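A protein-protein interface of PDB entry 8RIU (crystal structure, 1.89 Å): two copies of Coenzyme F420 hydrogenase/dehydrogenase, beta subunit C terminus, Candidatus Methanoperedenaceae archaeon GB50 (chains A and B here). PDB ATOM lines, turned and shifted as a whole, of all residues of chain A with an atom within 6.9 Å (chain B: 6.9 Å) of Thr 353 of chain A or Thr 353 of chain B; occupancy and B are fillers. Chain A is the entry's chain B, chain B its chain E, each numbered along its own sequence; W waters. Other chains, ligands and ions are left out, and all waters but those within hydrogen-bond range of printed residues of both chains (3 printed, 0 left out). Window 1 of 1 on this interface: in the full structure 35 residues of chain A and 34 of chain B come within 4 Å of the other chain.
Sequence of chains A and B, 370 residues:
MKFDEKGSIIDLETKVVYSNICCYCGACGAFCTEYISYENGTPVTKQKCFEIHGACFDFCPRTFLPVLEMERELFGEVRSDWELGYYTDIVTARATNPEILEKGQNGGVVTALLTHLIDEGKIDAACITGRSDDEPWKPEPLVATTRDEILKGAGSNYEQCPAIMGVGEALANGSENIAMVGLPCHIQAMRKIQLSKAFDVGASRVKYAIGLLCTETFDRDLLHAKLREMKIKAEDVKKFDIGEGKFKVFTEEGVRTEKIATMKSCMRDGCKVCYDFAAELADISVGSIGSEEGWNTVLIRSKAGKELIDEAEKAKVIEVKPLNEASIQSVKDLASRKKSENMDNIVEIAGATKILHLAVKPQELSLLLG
Phe 3 of chain A touches Ala 352 of chain B, and with the chains exchanged Ala 352 of chain A touches Phe 3 of chain B.
Ala 350 of chain A touches Leu 356 of chain B, and with the chains exchanged Leu 356 of chain A touches Ala 350 of chain B.
Thr 353 of chain A touches its own counterpart, Thr 353 of chain B.
Lys 354 of chain A touches Thr 353 of chain B, but with the chains exchanged Thr 353 of chain A does not touch Lys 354 of chain B (4.3 Å).
Of the 8 pairs that touch across the chains among the printed residues, 7 have their exchanged pair printed and touching as well.
Water W2 lies within hydrogen-bond range of N of Lys 354 of chain B (2.9 Å) and N of Lys 354 of chain A (3.1 Å).
Water W1 lies within hydrogen-bond range of the backbone NH (N) of Leu 356 of chain B and the backbone NH (N) of Gly 351 of chain A.
Water W3 bridges N of Leu 356 of chain A and N of Gly 351 of chain B.
Among the printed residues, merely in contact across the chains: Thr 353 of chain A with Thr 353 of chain B (3.5 Å), Lys 354 of chain A with Thr 353 of chain B (3.7 Å), Leu 356 of chain A with Ala 350 of chain B (3.7 Å), Ala 350 of chain A with Leu 356 of chain B (3.7 Å), Phe 3 of chain A with Ala 352 of chain B (3.8 Å), Lys 361 of chain A with Phe 3 of chain B (3.8 Å), Ala 352 of chain A with Phe 3 of chain B (3.9 Å) and Phe 3 of chain A with Lys 361 of chain B (3.9 Å).
Printed residues of chain A that touch a printed residue of chain B: Phe 3, Ala 350, Ala 352, Thr 353, Lys 354, Leu 356 and Lys 361.
Hydrophobic or aromatic side chains of chain A that line the printed part of chain B: Phe 3, Ala 350 and Ala 352.
Hydrophobic or aromatic side chains of chain B within 4 Å of the printed part of chain A: Phe 3, Ala 350 and Ala 352.
Among the printed residues, 8 pairs touch across the chains.
N of Thr 353 of chain A sits at hydrogen-bond distance from O of Val 360 of chain A, 2.6 Å away.
The backbone carbonyl oxygen (O) of Val 360 of chain B lies within hydrogen-bond range of the backbone NH (N) of Thr 353 of chain B (2.8 Å).
Printed residues of chain B within 4 Å of Ala 350 of chain A: Leu 356 (3.7 Å).
Thr 353 of chain A touches just one residue of chain B: Thr 353.
Of the printed residues of chain B, Leu 356 of chain A touches Ala 350.
Of the printed residues of chain A, Ala 352 of chain B touches Phe 3.
Of the printed residues of chain A, Thr 353 of chain B touches Thr 353 (3.5 Å) and Lys 354 (3.7 Å).
Of the printed residues of chain A, Lys 361 of chain B touches Phe 3 (3.9 Å).
The nearest residue of chain B that does not touch Thr 353 of chain A is Ile 355 of chain B (4.2 Å).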
ATOM      1  N   PHE A   3      -6.646 -10.748  -6.760  1.00  0.00           N
ATOM      2  CA  PHE A   3      -6.402  -9.470  -7.466  1.00  0.00           C
ATOM      3  C   PHE A   3      -7.558  -8.513  -7.179  1.00  0.00           C
ATOM      4  O   PHE A   3      -7.807  -7.624  -7.999  1.00  0.00           O
ATOM      5  CB  PHE A   3      -6.199  -9.711  -8.961  1.00  0.00           C
ATOM      6  CG  PHE A   3      -5.020 -10.582  -9.308  1.00  0.00           C
ATOM      7  CD1 PHE A   3      -3.952 -10.710  -8.436  1.00  0.00           C
ATOM      8  CD2 PHE A   3      -4.976 -11.269 -10.508  1.00  0.00           C
ATOM      9  CE1 PHE A   3      -2.869 -11.512  -8.755  1.00  0.00           C
ATOM     10  CE2 PHE A   3      -3.892 -12.069 -10.828  1.00  0.00           C
ATOM     11  CZ  PHE A   3      -2.841 -12.190  -9.950  1.00  0.00           C
ATOM     12  N   ALA A 350      -4.762   3.632 -20.982  1.00  0.00           N
ATOM     13  CA  ALA A 350      -4.098   2.873 -19.933  1.00  0.00           C
ATOM     14  C   ALA A 350      -2.769   3.508 -19.552  1.00  0.00           C
ATOM     15  O   ALA A 350      -2.087   4.126 -20.374  1.00  0.00           O
ATOM     16  CB  ALA A 350      -3.865   1.429 -20.385  1.00  0.00           C
ATOM     17  N   GLY A 351      -2.404   3.349 -18.282  1.00  0.00           N
ATOM     18  CA  GLY A 351      -1.084   3.714 -17.822  1.00  0.00           C
ATOM     19  C   GLY A 351      -0.043   2.697 -18.247  1.00  0.00           C
ATOM     20  O   GLY A 351      -0.327   1.700 -18.910  1.00  0.00           O
ATOM     21  N   ALA A 352       1.198   2.961 -17.851  1.00  0.00           N
ATOM     22  CA  ALA A 352       2.290   2.076 -18.227  1.00  0.00           C
ATOM     23  C   ALA A 352       2.002   0.657 -17.760  1.00  0.00           C
ATOM     24  O   ALA A 352       1.382   0.437 -16.718  1.00  0.00           O
ATOM     25  CB  ALA A 352       3.608   2.560 -17.625  1.00  0.00           C
ATOM     26  N   THR A 353       2.436  -0.313 -18.559  1.00  0.00           N
ATOM     27  CA  THR A 353       2.390  -1.713 -18.168  1.00  0.00           C
ATOM     28  C   THR A 353       3.699  -2.060 -17.474  1.00  0.00           C
ATOM     29  O   THR A 353       4.780  -1.804 -18.017  1.00  0.00           O
ATOM     30  CB  THR A 353       2.172  -2.613 -19.382  1.00  0.00           C
ATOM     31  OG1 THR A 353       1.022  -2.167 -20.117  1.00  0.00           O
ATOM     32  CG2 THR A 353       1.959  -4.047 -18.944  1.00  0.00           C
ATOM     33  N   LYS A 354       3.604  -2.626 -16.274  1.00  0.00           N
ATOM     34  CA  LYS A 354       4.776  -2.950 -15.474  1.00  0.00           C
ATOM     35  C   LYS A 354       4.882  -4.456 -15.284  1.00  0.00           C
ATOM     36  O   LYS A 354       3.902  -5.114 -14.919  1.00  0.00           O
ATOM     37  CB  LYS A 354       4.722  -2.256 -14.115  1.00  0.00           C
ATOM     38  CG  LYS A 354       6.066  -2.209 -13.402  1.00  0.00           C
ATOM     39  CD  LYS A 354       6.356  -0.830 -12.834  1.00  0.00           C
ATOM     40  CE  LYS A 354       7.795  -0.725 -12.348  1.00  0.00           C
ATOM     41  NZ  LYS A 354       7.871  -0.705 -10.862  1.00  0.00           N
ATOM     42  N   ILE A 355       6.081  -4.990 -15.524  1.00  0.00           N
ATOM     43  CA  ILE A 355       6.392  -6.407 -15.339  1.00  0.00           C
ATOM     44  C   ILE A 355       7.647  -6.455 -14.476  1.00  0.00           C
ATOM     45  O   ILE A 355       8.759  -6.224 -14.966  1.00  0.00           O
ATOM     46  CB  ILE A 355       6.593  -7.139 -16.670  1.00  0.00           C
ATOM     47  CG1 ILE A 355       5.384  -6.892 -17.577  1.00  0.00           C
ATOM     48  CG2 ILE A 355       6.795  -8.625 -16.435  1.00  0.00           C
ATOM     49  CD1 ILE A 355       5.481  -7.555 -18.936  1.00  0.00           C
ATOM     50  N   LEU A 356       7.472  -6.754 -13.188  1.00  0.00           N
ATOM     51  CA  LEU A 356       8.521  -6.571 -12.190  1.00  0.00           C
ATOM     52  C   LEU A 356       9.068  -5.142 -12.226  1.00  0.00           C
ATOM     53  O   LEU A 356       8.341  -4.196 -11.902  1.00  0.00           O
ATOM     54  CB  LEU A 356       9.626  -7.615 -12.380  1.00  0.00           C
ATOM     55  CG  LEU A 356      10.571  -7.821 -11.187  1.00  0.00           C
ATOM     56  CD1 LEU A 356       9.819  -8.314  -9.954  1.00  0.00           C
ATOM     57  CD2 LEU A 356      11.701  -8.789 -11.536  1.00  0.00           C
ATOM     58  N   LEU A 358      10.356  -3.766 -15.086  1.00  0.00           N
ATOM     59  CA  LEU A 358      10.223  -3.255 -16.444  1.00  0.00           C
ATOM     60  C   LEU A 358       8.899  -2.521 -16.614  1.00  0.00           C
ATOM     61  O   LEU A 358       7.846  -3.028 -16.215  1.00  0.00           O
ATOM     62  CB  LEU A 358      10.313  -4.410 -17.442  1.00  0.00           C
ATOM     63  CG  LEU A 358      11.587  -5.257 -17.374  1.00  0.00           C
ATOM     64  CD1 LEU A 358      11.379  -6.597 -18.052  1.00  0.00           C
ATOM     65  CD2 LEU A 358      12.747  -4.514 -18.016  1.00  0.00           C
ATOM     66  N   ALA A 359       8.952  -1.338 -17.227  1.00  0.00           N
ATOM     67  CA  ALA A 359       7.773  -0.511 -17.462  1.00  0.00           C
ATOM     68  C   ALA A 359       7.752  -0.058 -18.916  1.00  0.00           C
ATOM     69  O   ALA A 359       8.752   0.466 -19.419  1.00  0.00           O
ATOM     70  CB  ALA A 359       7.763   0.713 -16.537  1.00  0.00           C
ATOM     71  N   VAL A 360       6.612  -0.251 -19.584  1.00  0.00           N
ATOM     72  CA  VAL A 360       6.453   0.118 -20.984  1.00  0.00           C
ATOM     73  C   VAL A 360       5.039   0.630 -21.220  1.00  0.00           C
ATOM     74  O   VAL A 360       4.105   0.313 -20.481  1.00  0.00           O
ATOM     75  CB  VAL A 360       6.728  -1.069 -21.936  1.00  0.00           C
ATOM     76  CG1 VAL A 360       8.202  -1.412 -21.952  1.00  0.00           C
ATOM     77  CG2 VAL A 360       5.908  -2.269 -21.523  1.00  0.00           C
ATOM     78  N   LYS A 361       4.890   1.425 -22.274  1.00  0.00           N
ATOM     79  CA  LYS A 361       3.558   1.703 -22.788  1.00  0.00           C
ATOM     80  C   LYS A 361       2.897   0.382 -23.170  1.00  0.00           C
ATOM     81  O   LYS A 361       3.573  -0.520 -23.678  1.00  0.00           O
ATOM     82  CB  LYS A 361       3.623   2.622 -24.005  1.00  0.00           C
ATOM     83  CG  LYS A 361       3.848   4.088 -23.678  1.00  0.00           C
ATOM     84  CD  LYS A 361       4.409   4.828 -24.885  1.00  0.00           C
ATOM     85  CE  LYS A 361       4.266   6.338 -24.755  1.00  0.00           C
ATOM     86  NZ  LYS A 361       5.483   6.978 -24.169  1.00  0.00           N
ATOM     87  N   PRO A 362       1.591   0.220 -22.938  1.00  0.00           N
ATOM     88  CA  PRO A 362       0.970  -1.078 -23.247  1.00  0.00           C
ATOM     89  C   PRO A 362       1.071  -1.457 -24.714  1.00  0.00           C
ATOM     90  O   PRO A 362       1.290  -2.634 -25.028  1.00  0.00           O
ATOM     91  CB  PRO A 362      -0.490  -0.888 -22.806  1.00  0.00           C
ATOM     92  CG  PRO A 362      -0.468   0.263 -21.872  1.00  0.00           C
ATOM     93  CD  PRO A 362       0.619   1.167 -22.369  1.00  0.00           C
ATOM     94  N   GLN A 363       0.922  -0.494 -25.628  1.00  0.00           N
ATOM     95  CA  GLN A 363       0.985  -0.828 -27.048  1.00  0.00           C
ATOM     96  C   GLN A 363       2.394  -1.176 -27.506  1.00  0.00           C
ATOM     97  O   GLN A 363       2.564  -1.609 -28.649  1.00  0.00           O
ATOM     98  CB  GLN A 363       0.439   0.318 -27.908  1.00  0.00           C
ATOM     99  CG  GLN A 363       1.168   1.643 -27.792  1.00  0.00           C
ATOM    100  CD  GLN A 363       0.676   2.478 -26.629  1.00  0.00           C
ATOM    101  OE1 GLN A 363       0.638   2.011 -25.483  1.00  0.00           O
ATOM    102  NE2 GLN A 363       0.281   3.718 -26.914  1.00  0.00           N
ATOM    103  N   LEU A 365       4.257  -3.435 -25.728  1.00  0.00           N
ATOM    104  CA  LEU A 365       4.581  -4.693 -25.011  1.00  0.00           C
ATOM    105  C   LEU A 365       5.348  -5.644 -25.930  1.00  0.00           C
ATOM    106  O   LEU A 365       6.195  -6.387 -25.423  1.00  0.00           O
ATOM    107  CB  LEU A 365       3.271  -5.325 -24.539  1.00  0.00           C
ATOM    108  CG  LEU A 365       2.928  -5.115 -23.067  1.00  0.00           C
ATOM    109  CD1 LEU A 365       1.592  -5.758 -22.738  1.00  0.00           C
ATOM    110  CD2 LEU A 365       4.024  -5.675 -22.178  1.00  0.00           C
ATOM    111  N   LEU A 368       9.029  -5.085 -26.281  1.00  0.00           N
ATOM    112  CA  LEU A 368       9.797  -5.514 -25.122  1.00  0.00           C
ATOM    113  C   LEU A 368       9.835  -7.024 -24.981  1.00  0.00           C
ATOM    114  O   LEU A 368      10.849  -7.568 -24.536  1.00  0.00           O
ATOM    115  CB  LEU A 368       9.210  -4.892 -23.851  1.00  0.00           C
ATOM    116  CG  LEU A 368       9.767  -5.342 -22.502  1.00  0.00           C
ATOM    117  CD1 LEU A 368      10.979  -4.516 -22.124  1.00  0.00           C
ATOM    118  CD2 LEU A 368       8.693  -5.222 -21.439  1.00  0.00           C
ATOM    119  N   PHE B   3       7.746   7.658 -16.739  1.00  0.00           N
ATOM    120  CA  PHE B   3       7.485   6.427 -15.951  1.00  0.00           C
ATOM    121  C   PHE B   3       8.389   6.407 -14.716  1.00  0.00           C
ATOM    122  O   PHE B   3       8.629   5.336 -14.166  1.00  0.00           O
ATOM    123  CB  PHE B   3       7.635   5.205 -16.857  1.00  0.00           C
ATOM    124  CG  PHE B   3       6.687   5.194 -18.029  1.00  0.00           C
ATOM    125  CD1 PHE B   3       5.564   6.004 -18.039  1.00  0.00           C
ATOM    126  CD2 PHE B   3       6.938   4.406 -19.139  1.00  0.00           C
ATOM    127  CE1 PHE B   3       4.697   6.003 -19.119  1.00  0.00           C
ATOM    128  CE2 PHE B   3       6.073   4.410 -20.220  1.00  0.00           C
ATOM    129  CZ  PHE B   3       4.954   5.207 -20.208  1.00  0.00           C
ATOM    130  N   ALA B 350       6.896 -11.471 -10.276  1.00  0.00           N
ATOM    131  CA  ALA B 350       6.211 -10.240 -10.634  1.00  0.00           C
ATOM    132  C   ALA B 350       4.782 -10.248 -10.120  1.00  0.00           C
ATOM    133  O   ALA B 350       4.121 -11.287 -10.086  1.00  0.00           O
ATOM    134  CB  ALA B 350       6.215 -10.062 -12.151  1.00  0.00           C
ATOM    135  N   GLY B 351       4.307  -9.078  -9.715  1.00  0.00           N
ATOM    136  CA  GLY B 351       2.913  -8.915  -9.371  1.00  0.00           C
ATOM    137  C   GLY B 351       2.041  -8.983 -10.609  1.00  0.00           C
ATOM    138  O   GLY B 351       2.501  -9.175 -11.735  1.00  0.00           O
ATOM    139  N   ALA B 352       0.743  -8.821 -10.387  1.00  0.00           N
ATOM    140  CA  ALA B 352      -0.201  -8.861 -11.492  1.00  0.00           C
ATOM    141  C   ALA B 352       0.088  -7.741 -12.480  1.00  0.00           C
ATOM    142  O   ALA B 352       0.479  -6.634 -12.100  1.00  0.00           O
ATOM    143  CB  ALA B 352      -1.632  -8.740 -10.973  1.00  0.00           C
ATOM    144  N   THR B 353      -0.100  -8.039 -13.760  1.00  0.00           N
ATOM    145  CA  THR B 353       0.020  -7.050 -14.821  1.00  0.00           C
ATOM    146  C   THR B 353      -1.356  -6.453 -15.076  1.00  0.00           C
ATOM    147  O   THR B 353      -2.334  -7.194 -15.232  1.00  0.00           O
ATOM    148  CB  THR B 353       0.568  -7.697 -16.095  1.00  0.00           C
ATOM    149  OG1 THR B 353       1.941  -8.059 -15.897  1.00  0.00           O
ATOM    150  CG2 THR B 353       0.468  -6.744 -17.281  1.00  0.00           C
ATOM    151  N   LYS B 354      -1.434  -5.122 -15.117  1.00  0.00           N
ATOM    152  CA  LYS B 354      -2.701  -4.428 -15.316  1.00  0.00           C
ATOM    153  C   LYS B 354      -2.667  -3.599 -16.594  1.00  0.00           C
ATOM    154  O   LYS B 354      -1.720  -2.840 -16.828  1.00  0.00           O
ATOM    155  CB  LYS B 354      -3.035  -3.529 -14.127  1.00  0.00           C
ATOM    156  CG  LYS B 354      -3.603  -4.290 -12.934  1.00  0.00           C
ATOM    157  CD  LYS B 354      -4.509  -3.420 -12.042  1.00  0.00           C
ATOM    158  CE  LYS B 354      -5.652  -2.763 -12.817  1.00  0.00           C
ATOM    159  NZ  LYS B 354      -6.744  -2.266 -11.922  1.00  0.00           N
ATOM    160  N   ILE B 355      -3.714  -3.749 -17.404  1.00  0.00           N
ATOM    161  CA  ILE B 355      -3.904  -2.997 -18.641  1.00  0.00           C
ATOM    162  C   ILE B 355      -5.292  -2.379 -18.542  1.00  0.00           C
ATOM    163  O   ILE B 355      -6.297  -3.043 -18.830  1.00  0.00           O
ATOM    164  CB  ILE B 355      -3.773  -3.877 -19.886  1.00  0.00           C
ATOM    165  CG1 ILE B 355      -2.390  -4.526 -19.916  1.00  0.00           C
ATOM    166  CG2 ILE B 355      -4.002  -3.049 -21.143  1.00  0.00           C
ATOM    167  CD1 ILE B 355      -2.246  -5.624 -20.942  1.00  0.00           C
ATOM    168  N   LEU B 356      -5.356  -1.111 -18.136  1.00  0.00           N
ATOM    169  CA  LEU B 356      -6.615  -0.439 -17.797  1.00  0.00           C
ATOM    170  C   LEU B 356      -7.272  -1.322 -16.743  1.00  0.00           C
ATOM    171  O   LEU B 356      -6.610  -1.649 -15.742  1.00  0.00           O
ATOM    172  CB  LEU B 356      -7.435  -0.202 -19.068  1.00  0.00           C
ATOM    173  CG  LEU B 356      -8.547   0.852 -18.960  1.00  0.00           C
ATOM    174  CD1 LEU B 356      -7.981   2.247 -18.722  1.00  0.00           C
ATOM    175  CD2 LEU B 356      -9.440   0.846 -20.202  1.00  0.00           C
ATOM    176  N   LEU B 358      -8.160  -4.483 -16.920  1.00  0.00           N
ATOM    177  CA  LEU B 358      -7.816  -5.893 -17.000  1.00  0.00           C
ATOM    178  C   LEU B 358      -6.590  -6.186 -16.149  1.00  0.00           C
ATOM    179  O   LEU B 358      -5.628  -5.413 -16.132  1.00  0.00           O
ATOM    180  CB  LEU B 358      -7.560  -6.298 -18.452  1.00  0.00           C
ATOM    181  CG  LEU B 358      -8.752  -6.109 -19.393  1.00  0.00           C
ATOM    182  CD1 LEU B 358      -8.293  -6.089 -20.837  1.00  0.00           C
ATOM    183  CD2 LEU B 358      -9.788  -7.205 -19.181  1.00  0.00           C
ATOM    184  N   ALA B 359      -6.631  -7.308 -15.438  1.00  0.00           N
ATOM    185  CA  ALA B 359      -5.518  -7.728 -14.598  1.00  0.00           C
ATOM    186  C   ALA B 359      -5.305  -9.215 -14.798  1.00  0.00           C
ATOM    187  O   ALA B 359      -6.258  -9.993 -14.703  1.00  0.00           O
ATOM    188  CB  ALA B 359      -5.779  -7.421 -13.119  1.00  0.00           C
ATOM    189  N   VAL B 360      -4.063  -9.604 -15.082  1.00  0.00           N
ATOM    190  CA  VAL B 360      -3.710 -11.005 -15.265  1.00  0.00           C
ATOM    191  C   VAL B 360      -2.300 -11.224 -14.735  1.00  0.00           C
ATOM    192  O   VAL B 360      -1.493 -10.295 -14.648  1.00  0.00           O
ATOM    193  CB  VAL B 360      -3.788 -11.444 -16.747  1.00  0.00           C
ATOM    194  CG1 VAL B 360      -5.200 -11.260 -17.293  1.00  0.00           C
ATOM    195  CG2 VAL B 360      -2.783 -10.668 -17.582  1.00  0.00           C
ATOM    196  N   LYS B 361      -2.007 -12.472 -14.389  1.00  0.00           N
ATOM    197  CA  LYS B 361      -0.636 -12.850 -14.097  1.00  0.00           C
ATOM    198  C   LYS B 361       0.232 -12.566 -15.320  1.00  0.00           C
ATOM    199  O   LYS B 361      -0.195 -12.821 -16.453  1.00  0.00           O
ATOM    200  CB  LYS B 361      -0.549 -14.333 -13.735  1.00  0.00           C
ATOM    201  CG  LYS B 361      -1.415 -14.752 -12.560  1.00  0.00           C
ATOM    202  CD  LYS B 361      -0.616 -15.585 -11.565  1.00  0.00           C
ATOM    203  CE  LYS B 361      -1.508 -16.469 -10.709  1.00  0.00           C
ATOM    204  NZ  LYS B 361      -2.373 -17.369 -11.522  1.00  0.00           N
ATOM    205  N   PRO B 362       1.439 -12.021 -15.140  1.00  0.00           N
ATOM    206  CA  PRO B 362       2.303 -11.784 -16.309  1.00  0.00           C
ATOM    207  C   PRO B 362       2.495 -13.015 -17.181  1.00  0.00           C
ATOM    208  O   PRO B 362       2.539 -12.891 -18.411  1.00  0.00           O
ATOM    209  CB  PRO B 362       3.627 -11.323 -15.683  1.00  0.00           C
ATOM    210  CG  PRO B 362       3.271 -10.791 -14.336  1.00  0.00           C
ATOM    211  CD  PRO B 362       1.952 -11.379 -13.917  1.00  0.00           C
ATOM    212  N   GLN B 363       2.605 -14.204 -16.583  1.00  0.00           N
ATOM    213  CA  GLN B 363       2.837 -15.405 -17.377  1.00  0.00           C
ATOM    214  C   GLN B 363       1.638 -15.776 -18.245  1.00  0.00           C
ATOM    215  O   GLN B 363       1.814 -16.473 -19.248  1.00  0.00           O
ATOM    216  CB  GLN B 363       3.211 -16.577 -16.463  1.00  0.00           C
ATOM    217  CG  GLN B 363       2.122 -17.010 -15.492  1.00  0.00           C
ATOM    218  CD  GLN B 363       2.538 -18.176 -14.606  1.00  0.00           C
ATOM    219  OE1 GLN B 363       3.730 -18.451 -14.430  1.00  0.00           O
ATOM    220  NE2 GLN B 363       1.550 -18.859 -14.030  1.00  0.00           N
ATOM    221  N   LEU B 365      -0.166 -13.622 -19.888  1.00  0.00           N
ATOM    222  CA  LEU B 365      -0.450 -12.432 -20.680  1.00  0.00           C
ATOM    223  C   LEU B 365      -0.960 -12.797 -22.069  1.00  0.00           C
ATOM    224  O   LEU B 365      -1.892 -12.166 -22.581  1.00  0.00           O
ATOM    225  CB  LEU B 365       0.816 -11.585 -20.767  1.00  0.00           C
ATOM    226  CG  LEU B 365       0.683 -10.097 -21.051  1.00  0.00           C
ATOM    227  CD1 LEU B 365      -0.197  -9.407 -20.027  1.00  0.00           C
ATOM    228  CD2 LEU B 365       2.084  -9.494 -21.050  1.00  0.00           C
ATOM    229  N   LEU B 368      -4.625 -13.662 -22.545  1.00  0.00           N
ATOM    230  CA  LEU B 368      -5.519 -12.517 -22.600  1.00  0.00           C
ATOM    231  C   LEU B 368      -5.395 -11.770 -23.924  1.00  0.00           C
ATOM    232  O   LEU B 368      -6.406 -11.349 -24.498  1.00  0.00           O
ATOM    233  CB  LEU B 368      -5.220 -11.574 -21.428  1.00  0.00           C
ATOM    234  CG  LEU B 368      -5.985 -10.249 -21.373  1.00  0.00           C
ATOM    235  CD1 LEU B 368      -7.425 -10.484 -20.955  1.00  0.00           C
ATOM    236  CD2 LEU B 368      -5.306  -9.279 -20.426  1.00  0.00           C
HETATM  237  O   HOH W   1      -3.419   0.806 -16.893  1.00  0.00           O
HETATM  238  O   HOH W   2       0.842  -3.355 -15.002  1.00  0.00           O
HETATM  239  O   HOH W   3       4.917  -6.676 -11.528  1.00  0.00           O
